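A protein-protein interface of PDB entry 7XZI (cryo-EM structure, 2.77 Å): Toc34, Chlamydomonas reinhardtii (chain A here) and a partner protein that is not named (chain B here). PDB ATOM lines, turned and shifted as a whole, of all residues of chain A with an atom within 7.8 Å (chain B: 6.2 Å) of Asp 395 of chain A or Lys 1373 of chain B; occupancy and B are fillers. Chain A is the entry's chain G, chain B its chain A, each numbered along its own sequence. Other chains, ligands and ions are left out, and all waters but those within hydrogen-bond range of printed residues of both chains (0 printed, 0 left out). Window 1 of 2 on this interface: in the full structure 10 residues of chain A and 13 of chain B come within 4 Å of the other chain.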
ATOM      1  N   GLU A 360      14.947  -6.613 -15.438  1.00  0.00           N
ATOM      2  CA  GLU A 360      13.624  -6.122 -15.072  1.00  0.00           C
ATOM      3  C   GLU A 360      13.479  -4.655 -15.445  1.00  0.00           C
ATOM      4  O   GLU A 360      12.501  -4.261 -16.096  1.00  0.00           O
ATOM      5  CB  GLU A 360      13.385  -6.340 -13.576  1.00  0.00           C
ATOM      6  CG  GLU A 360      12.025  -5.878 -13.075  1.00  0.00           C
ATOM      7  CD  GLU A 360      12.049  -4.465 -12.526  1.00  0.00           C
ATOM      8  OE1 GLU A 360      13.142  -3.861 -12.481  1.00  0.00           O
ATOM      9  OE2 GLU A 360      10.976  -3.960 -12.135  1.00  0.00           O
ATOM     10  N   TRP A 364      10.599  -2.270 -18.034  1.00  0.00           N
ATOM     11  CA  TRP A 364       9.852  -1.054 -17.743  1.00  0.00           C
ATOM     12  C   TRP A 364      10.207   0.053 -18.719  1.00  0.00           C
ATOM     13  O   TRP A 364       9.317   0.779 -19.179  1.00  0.00           O
ATOM     14  CB  TRP A 364      10.096  -0.605 -16.303  1.00  0.00           C
ATOM     15  CG  TRP A 364       9.270  -1.352 -15.303  1.00  0.00           C
ATOM     16  CD1 TRP A 364       9.712  -2.271 -14.397  1.00  0.00           C
ATOM     17  CD2 TRP A 364       7.853  -1.252 -15.113  1.00  0.00           C
ATOM     18  NE1 TRP A 364       8.659  -2.745 -13.651  1.00  0.00           N
ATOM     19  CE2 TRP A 364       7.507  -2.134 -14.072  1.00  0.00           C
ATOM     20  CE3 TRP A 364       6.844  -0.497 -15.721  1.00  0.00           C
ATOM     21  CZ2 TRP A 364       6.195  -2.286 -13.625  1.00  0.00           C
ATOM     22  CZ3 TRP A 364       5.543  -0.650 -15.276  1.00  0.00           C
ATOM     23  CH2 TRP A 364       5.230  -1.536 -14.239  1.00  0.00           C
ATOM     24  N   ARG A 367       8.164  -0.399 -21.631  1.00  0.00           N
ATOM     25  CA  ARG A 367       6.811   0.035 -21.310  1.00  0.00           C
ATOM     26  C   ARG A 367       6.694   1.548 -21.406  1.00  0.00           C
ATOM     27  O   ARG A 367       5.703   2.070 -21.933  1.00  0.00           O
ATOM     28  CB  ARG A 367       6.415  -0.449 -19.916  1.00  0.00           C
ATOM     29  CG  ARG A 367       6.380  -1.961 -19.767  1.00  0.00           C
ATOM     30  CD  ARG A 367       5.319  -2.588 -20.659  1.00  0.00           C
ATOM     31  NE  ARG A 367       3.979  -2.118 -20.332  1.00  0.00           N
ATOM     32  CZ  ARG A 367       3.197  -2.660 -19.404  1.00  0.00           C
ATOM     33  NH1 ARG A 367       3.594  -3.697 -18.685  1.00  0.00           N
ATOM     34  NH2 ARG A 367       1.990  -2.146 -19.193  1.00  0.00           N
ATOM     35  N   PRO A 382       4.765   0.141  -9.429  1.00  0.00           N
ATOM     36  CA  PRO A 382       4.855   0.078  -7.966  1.00  0.00           C
ATOM     37  C   PRO A 382       6.287   0.235  -7.480  1.00  0.00           C
ATOM     38  O   PRO A 382       7.255   0.090  -8.230  1.00  0.00           O
ATOM     39  CB  PRO A 382       4.312  -1.318  -7.633  1.00  0.00           C
ATOM     40  CG  PRO A 382       3.592  -1.772  -8.870  1.00  0.00           C
ATOM     41  CD  PRO A 382       4.323  -1.136 -10.008  1.00  0.00           C
ATOM     42  N   ALA A 386       6.610  -2.706  -2.586  1.00  0.00           N
ATOM     43  CA  ALA A 386       5.474  -3.472  -3.084  1.00  0.00           C
ATOM     44  C   ALA A 386       5.938  -4.625  -3.965  1.00  0.00           C
ATOM     45  O   ALA A 386       5.297  -5.679  -4.004  1.00  0.00           O
ATOM     46  CB  ALA A 386       4.518  -2.558  -3.851  1.00  0.00           C
ATOM     47  N   ALA A 387       7.055  -4.443  -4.675  1.00  0.00           N
ATOM     48  CA  ALA A 387       7.517  -5.459  -5.618  1.00  0.00           C
ATOM     49  C   ALA A 387       7.962  -6.736  -4.909  1.00  0.00           C
ATOM     50  O   ALA A 387       7.586  -7.843  -5.317  1.00  0.00           O
ATOM     51  CB  ALA A 387       8.653  -4.898  -6.475  1.00  0.00           C
ATOM     52  N   TRP A 388       8.777  -6.609  -3.857  1.00  0.00           N
ATOM     53  CA  TRP A 388       9.259  -7.807  -3.174  1.00  0.00           C
ATOM     54  C   TRP A 388       8.117  -8.530  -2.470  1.00  0.00           C
ATOM     55  O   TRP A 388       8.147  -9.757  -2.322  1.00  0.00           O
ATOM     56  CB  TRP A 388      10.380  -7.464  -2.188  1.00  0.00           C
ATOM     57  CG  TRP A 388       9.956  -6.727  -0.951  1.00  0.00           C
ATOM     58  CD1 TRP A 388      10.060  -5.390  -0.726  1.00  0.00           C
ATOM     59  CD2 TRP A 388       9.391  -7.291   0.241  1.00  0.00           C
ATOM     60  NE1 TRP A 388       9.581  -5.077   0.523  1.00  0.00           N
ATOM     61  CE2 TRP A 388       9.164  -6.228   1.138  1.00  0.00           C
ATOM     62  CE3 TRP A 388       9.047  -8.588   0.634  1.00  0.00           C
ATOM     63  CZ2 TRP A 388       8.612  -6.422   2.402  1.00  0.00           C
ATOM     64  CZ3 TRP A 388       8.498  -8.778   1.887  1.00  0.00           C
ATOM     65  CH2 TRP A 388       8.286  -7.702   2.756  1.00  0.00           C
ATOM     66  N   ARG A 389       7.107  -7.785  -2.014  1.00  0.00           N
ATOM     67  CA  ARG A 389       5.905  -8.427  -1.492  1.00  0.00           C
ATOM     68  C   ARG A 389       5.140  -9.139  -2.601  1.00  0.00           C
ATOM     69  O   ARG A 389       4.620 -10.242  -2.399  1.00  0.00           O
ATOM     70  CB  ARG A 389       5.017  -7.396  -0.797  1.00  0.00           C
ATOM     71  CG  ARG A 389       5.666  -6.719   0.400  1.00  0.00           C
ATOM     72  CD  ARG A 389       4.632  -6.006   1.252  1.00  0.00           C
ATOM     73  NE  ARG A 389       3.660  -6.938   1.807  1.00  0.00           N
ATOM     74  CZ  ARG A 389       2.604  -6.582   2.530  1.00  0.00           C
ATOM     75  NH1 ARG A 389       2.349  -5.313   2.804  1.00  0.00           N
ATOM     76  NH2 ARG A 389       1.783  -7.524   2.985  1.00  0.00           N
ATOM     77  N   LEU A 390       5.062  -8.519  -3.783  1.00  0.00           N
ATOM     78  CA  LEU A 390       4.405  -9.134  -4.929  1.00  0.00           C
ATOM     79  C   LEU A 390       5.145 -10.367  -5.422  1.00  0.00           C
ATOM     80  O   LEU A 390       4.562 -11.172  -6.158  1.00  0.00           O
ATOM     81  CB  LEU A 390       4.270  -8.120  -6.065  1.00  0.00           C
ATOM     82  N   GLU A 391       6.419 -10.520  -5.055  1.00  0.00           N
ATOM     83  CA  GLU A 391       7.117 -11.770  -5.342  1.00  0.00           C
ATOM     84  C   GLU A 391       6.404 -12.951  -4.693  1.00  0.00           C
ATOM     85  O   GLU A 391       6.302 -14.028  -5.291  1.00  0.00           O
ATOM     86  CB  GLU A 391       8.570 -11.681  -4.872  1.00  0.00           C
ATOM     87  CG  GLU A 391       9.364 -12.977  -5.008  1.00  0.00           C
ATOM     88  CD  GLU A 391       9.303 -13.844  -3.761  1.00  0.00           C
ATOM     89  OE1 GLU A 391       8.815 -13.358  -2.718  1.00  0.00           O
ATOM     90  OE2 GLU A 391       9.743 -15.011  -3.824  1.00  0.00           O
ATOM     91  N   GLN A 392       5.905 -12.766  -3.467  1.00  0.00           N
ATOM     92  CA  GLN A 392       5.138 -13.819  -2.807  1.00  0.00           C
ATOM     93  C   GLN A 392       3.806 -14.069  -3.501  1.00  0.00           C
ATOM     94  O   GLN A 392       3.222 -15.149  -3.354  1.00  0.00           O
ATOM     95  CB  GLN A 392       4.905 -13.461  -1.339  1.00  0.00           C
ATOM     96  CG  GLN A 392       6.102 -13.698  -0.438  1.00  0.00           C
ATOM     97  CD  GLN A 392       6.324 -15.167  -0.133  1.00  0.00           C
ATOM     98  OE1 GLN A 392       5.481 -16.012  -0.436  1.00  0.00           O
ATOM     99  NE2 GLN A 392       7.462 -15.477   0.474  1.00  0.00           N
ATOM    100  N   MET A 393       3.307 -13.091  -4.251  1.00  0.00           N
ATOM    101  CA  MET A 393       2.024 -13.217  -4.931  1.00  0.00           C
ATOM    102  C   MET A 393       2.178 -14.071  -6.189  1.00  0.00           C
ATOM    103  O   MET A 393       3.143 -14.825  -6.350  1.00  0.00           O
ATOM    104  N   TYR A 394       1.197 -13.979  -7.091  1.00  0.00           N
ATOM    105  CA  TYR A 394       1.275 -14.712  -8.350  1.00  0.00           C
ATOM    106  C   TYR A 394       2.438 -14.224  -9.205  1.00  0.00           C
ATOM    107  O   TYR A 394       2.944 -14.962 -10.058  1.00  0.00           O
ATOM    108  CB  TYR A 394      -0.045 -14.585  -9.112  1.00  0.00           C
ATOM    109  N   ASP A 395       2.870 -12.984  -8.994  1.00  0.00           N
ATOM    110  CA  ASP A 395       3.990 -12.414  -9.736  1.00  0.00           C
ATOM    111  C   ASP A 395       5.303 -13.097  -9.366  1.00  0.00           C
ATOM    112  O   ASP A 395       6.338 -12.444  -9.226  1.00  0.00           O
ATOM    113  CB  ASP A 395       4.087 -10.907  -9.480  1.00  0.00           C
ATOM    114  CG  ASP A 395       2.875 -10.150  -9.990  1.00  0.00           C
ATOM    115  OD1 ASP A 395       2.004 -10.784 -10.620  1.00  0.00           O
ATOM    116  OD2 ASP A 395       2.793  -8.924  -9.761  1.00  0.00           O
ATOM    117  N   THR B1371      -3.452 -11.482 -10.525  1.00  0.00           N
ATOM    118  CA  THR B1371      -2.215 -10.714 -10.467  1.00  0.00           C
ATOM    119  C   THR B1371      -1.227 -11.244 -11.501  1.00  0.00           C
ATOM    120  O   THR B1371      -0.902 -12.435 -11.508  1.00  0.00           O
ATOM    121  CB  THR B1371      -1.608 -10.785  -9.067  1.00  0.00           C
ATOM    122  OG1 THR B1371      -2.631 -10.553  -8.090  1.00  0.00           O
ATOM    123  CG2 THR B1371      -0.525  -9.733  -8.905  1.00  0.00           C
ATOM    124  N   ARG B1372      -0.749 -10.356 -12.370  1.00  0.00           N
ATOM    125  CA  ARG B1372       0.170 -10.721 -13.439  1.00  0.00           C
ATOM    126  C   ARG B1372       1.343  -9.754 -13.460  1.00  0.00           C
ATOM    127  O   ARG B1372       1.180  -8.559 -13.199  1.00  0.00           O
ATOM    128  CB  ARG B1372      -0.533 -10.721 -14.802  1.00  0.00           C
ATOM    129  N   LYS B1373       2.527 -10.280 -13.775  1.00  0.00           N
ATOM    130  CA  LYS B1373       3.740  -9.481 -13.834  1.00  0.00           C
ATOM    131  C   LYS B1373       4.178  -9.294 -15.278  1.00  0.00           C
ATOM    132  O   LYS B1373       4.187 -10.264 -16.049  1.00  0.00           O
ATOM    133  CB  LYS B1373       4.866 -10.141 -13.027  1.00  0.00           C
ATOM    134  CG  LYS B1373       5.150 -11.588 -13.402  1.00  0.00           C
ATOM    135  CD  LYS B1373       6.329 -12.142 -12.619  1.00  0.00           C
ATOM    136  CE  LYS B1373       7.595 -11.345 -12.887  1.00  0.00           C
ATOM    137  NZ  LYS B1373       7.980 -11.377 -14.325  1.00  0.00           N
ATOM    138  N   PRO B1374       4.523  -8.073 -15.688  1.00  0.00           N
ATOM    139  CA  PRO B1374       5.022  -7.872 -17.052  1.00  0.00           C
ATOM    140  C   PRO B1374       6.345  -8.590 -17.266  1.00  0.00           C
ATOM    141  O   PRO B1374       7.146  -8.755 -16.343  1.00  0.00           O
ATOM    142  CB  PRO B1374       5.184  -6.352 -17.151  1.00  0.00           C
ATOM    143  CG  PRO B1374       5.355  -5.900 -15.739  1.00  0.00           C
ATOM    144  CD  PRO B1374       4.507  -6.823 -14.911  1.00  0.00           C
ATOM    145  N   ARG B1375       6.570  -9.021 -18.505  1.00  0.00           N
ATOM    146  CA  ARG B1375       7.765  -9.776 -18.848  1.00  0.00           C
ATOM    147  C   ARG B1375       8.087  -9.551 -20.318  1.00  0.00           C
ATOM    148  O   ARG B1375       7.258  -9.069 -21.093  1.00  0.00           O
ATOM    149  CB  ARG B1375       7.584 -11.269 -18.554  1.00  0.00           C
ATOM    150  CG  ARG B1375       6.746 -11.997 -19.592  1.00  0.00           C
ATOM    151  CD  ARG B1375       5.866 -13.058 -18.954  1.00  0.00           C
ATOM    152  NE  ARG B1375       4.852 -12.466 -18.092  1.00  0.00           N
ATOM    153  CZ  ARG B1375       3.881 -13.150 -17.496  1.00  0.00           C
ATOM    154  NH1 ARG B1375       3.761 -14.458 -17.649  1.00  0.00           N
ATOM    155  NH2 ARG B1375       3.008 -12.502 -16.731  1.00  0.00           N
ATOM    156  N   LYS B1384       5.148  -8.518 -22.760  1.00  0.00           N
ATOM    157  CA  LYS B1384       4.059  -9.494 -22.744  1.00  0.00           C
ATOM    158  C   LYS B1384       3.447  -9.523 -21.346  1.00  0.00           C
ATOM    159  O   LYS B1384       3.931 -10.244 -20.469  1.00  0.00           O
ATOM    160  CB  LYS B1384       4.552 -10.872 -23.161  1.00  0.00           C
ATOM    161  N   ILE B1385       2.390  -8.740 -21.152  1.00  0.00           N
ATOM    162  CA  ILE B1385       1.508  -8.855 -19.998  1.00  0.00           C
ATOM    163  C   ILE B1385       0.105  -9.098 -20.538  1.00  0.00           C
ATOM    164  O   ILE B1385      -0.448  -8.245 -21.244  1.00  0.00           O
ATOM    165  CB  ILE B1385       1.558  -7.608 -19.100  1.00  0.00           C
ATOM    166  CG1 ILE B1385       0.363  -7.584 -18.144  1.00  0.00           C
ATOM    167  CG2 ILE B1385       1.630  -6.334 -19.936  1.00  0.00           C
ATOM    168  N   HIS B1430       5.683 -19.282  -4.140  1.00  0.00           N
ATOM    169  CA  HIS B1430       4.393 -18.626  -3.932  1.00  0.00           C
ATOM    170  C   HIS B1430       3.682 -19.208  -2.712  1.00  0.00           C
ATOM    171  O   HIS B1430       2.523 -19.625  -2.772  1.00  0.00           O
ATOM    172  CB  HIS B1430       3.515 -18.722  -5.182  1.00  0.00           C
ATOM    173  CG  HIS B1430       4.069 -17.995  -6.368  1.00  0.00           C
ATOM    174  ND1 HIS B1430       5.162 -17.161  -6.286  1.00  0.00           N
ATOM    175  CD2 HIS B1430       3.680 -17.978  -7.664  1.00  0.00           C
ATOM    176  CE1 HIS B1430       5.424 -16.661  -7.480  1.00  0.00           C
ATOM    177  NE2 HIS B1430       4.538 -17.140  -8.335  1.00  0.00           N
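A ring nitrogen (ND1) of His 1430 of chain B sits at hydrogen-bond distance from the backbone carbonyl oxygen of Met 393 of chain A. The side-chain carboxylate (OD1) of Asp 395 of chain A sits close to the backbone NH (N) of Arg 1372 of chain B (3.3 Å). The backbone carbonyl oxygen (O) of Tyr 394 of chain A is in hydrogen-bond range of a ring nitrogen (NE2) of His 1430 of chain B. O of Glu 391 of chain A lies within hydrogen-bond range of ND1 of His 1430 of chain B, 3.5 Å away. The side-chain carboxylate (OD1) of Asp 395 of chain A sits at hydrogen-bond distance from the backbone NH (N) of Lys 1373 of chain B, at 3.2 Å. OD1 of Asp 395 of chain A lies close to O of Thr 1371 of chain B.
The guanidinium group (NH2) of Arg 1375 of chain B lies within hydrogen-bond range of the backbone carbonyl oxygen (O) of Lys 1373 of chain B, at 2.6 Å.
Of the 14 printed residues of chain A, 6 touch a printed residue of chain B. Printed residues of chain B that touch a printed residue of chain A: Thr 1371, Arg 1372, Lys 1373, Pro 1374, Ile 1385 and His 1430. Among the printed residues, 10 pairs touch across the chains. Among the printed residues, no Asp or Glu carboxylate lies within 4 Å of a Lys or Arg side-chain nitrogen of the other chain.
Among the printed residues, merely in contact across the chains: Arg 367 of chain A with Pro 1374 of chain B (3.5 Å), Arg 367 of chain A with Ile 1385 of chain B (3.5 Å), Gln 392 of chain A with His 1430 of chain B (3.7 Å) and Tyr 394 of chain A with Thr 1371 of chain B (3.3 Å).
Trp 364 of chain A touches none of the printed residues of chain B. Of the printed residues of chain B, Arg 367 of chain A touches Pro 1374 and Ile 1385. Ala 386 of chain A touches none of the printed residues of chain B. Of the printed residues of chain B, Glu 391 of chain A touches His 1430 (3.5 Å). Printed residues of chain B within 4 Å of Gln 392 of chain A: His 1430 (3.7 Å). Asp 395 of chain A touches just these residues of chain B: Thr 1371, Arg 1372 and Lys 1373. Of the printed residues of chain A, Thr 1371 of chain B touches Tyr 394 and Asp 395. Of chain A, only Asp 395 (3.2 Å) comes within 4 Å of Lys 1373 of chain B. Of the printed residues of chain A, His 1430 of chain B touches Glu 391, Gln 392, Met 393 and Tyr 394.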
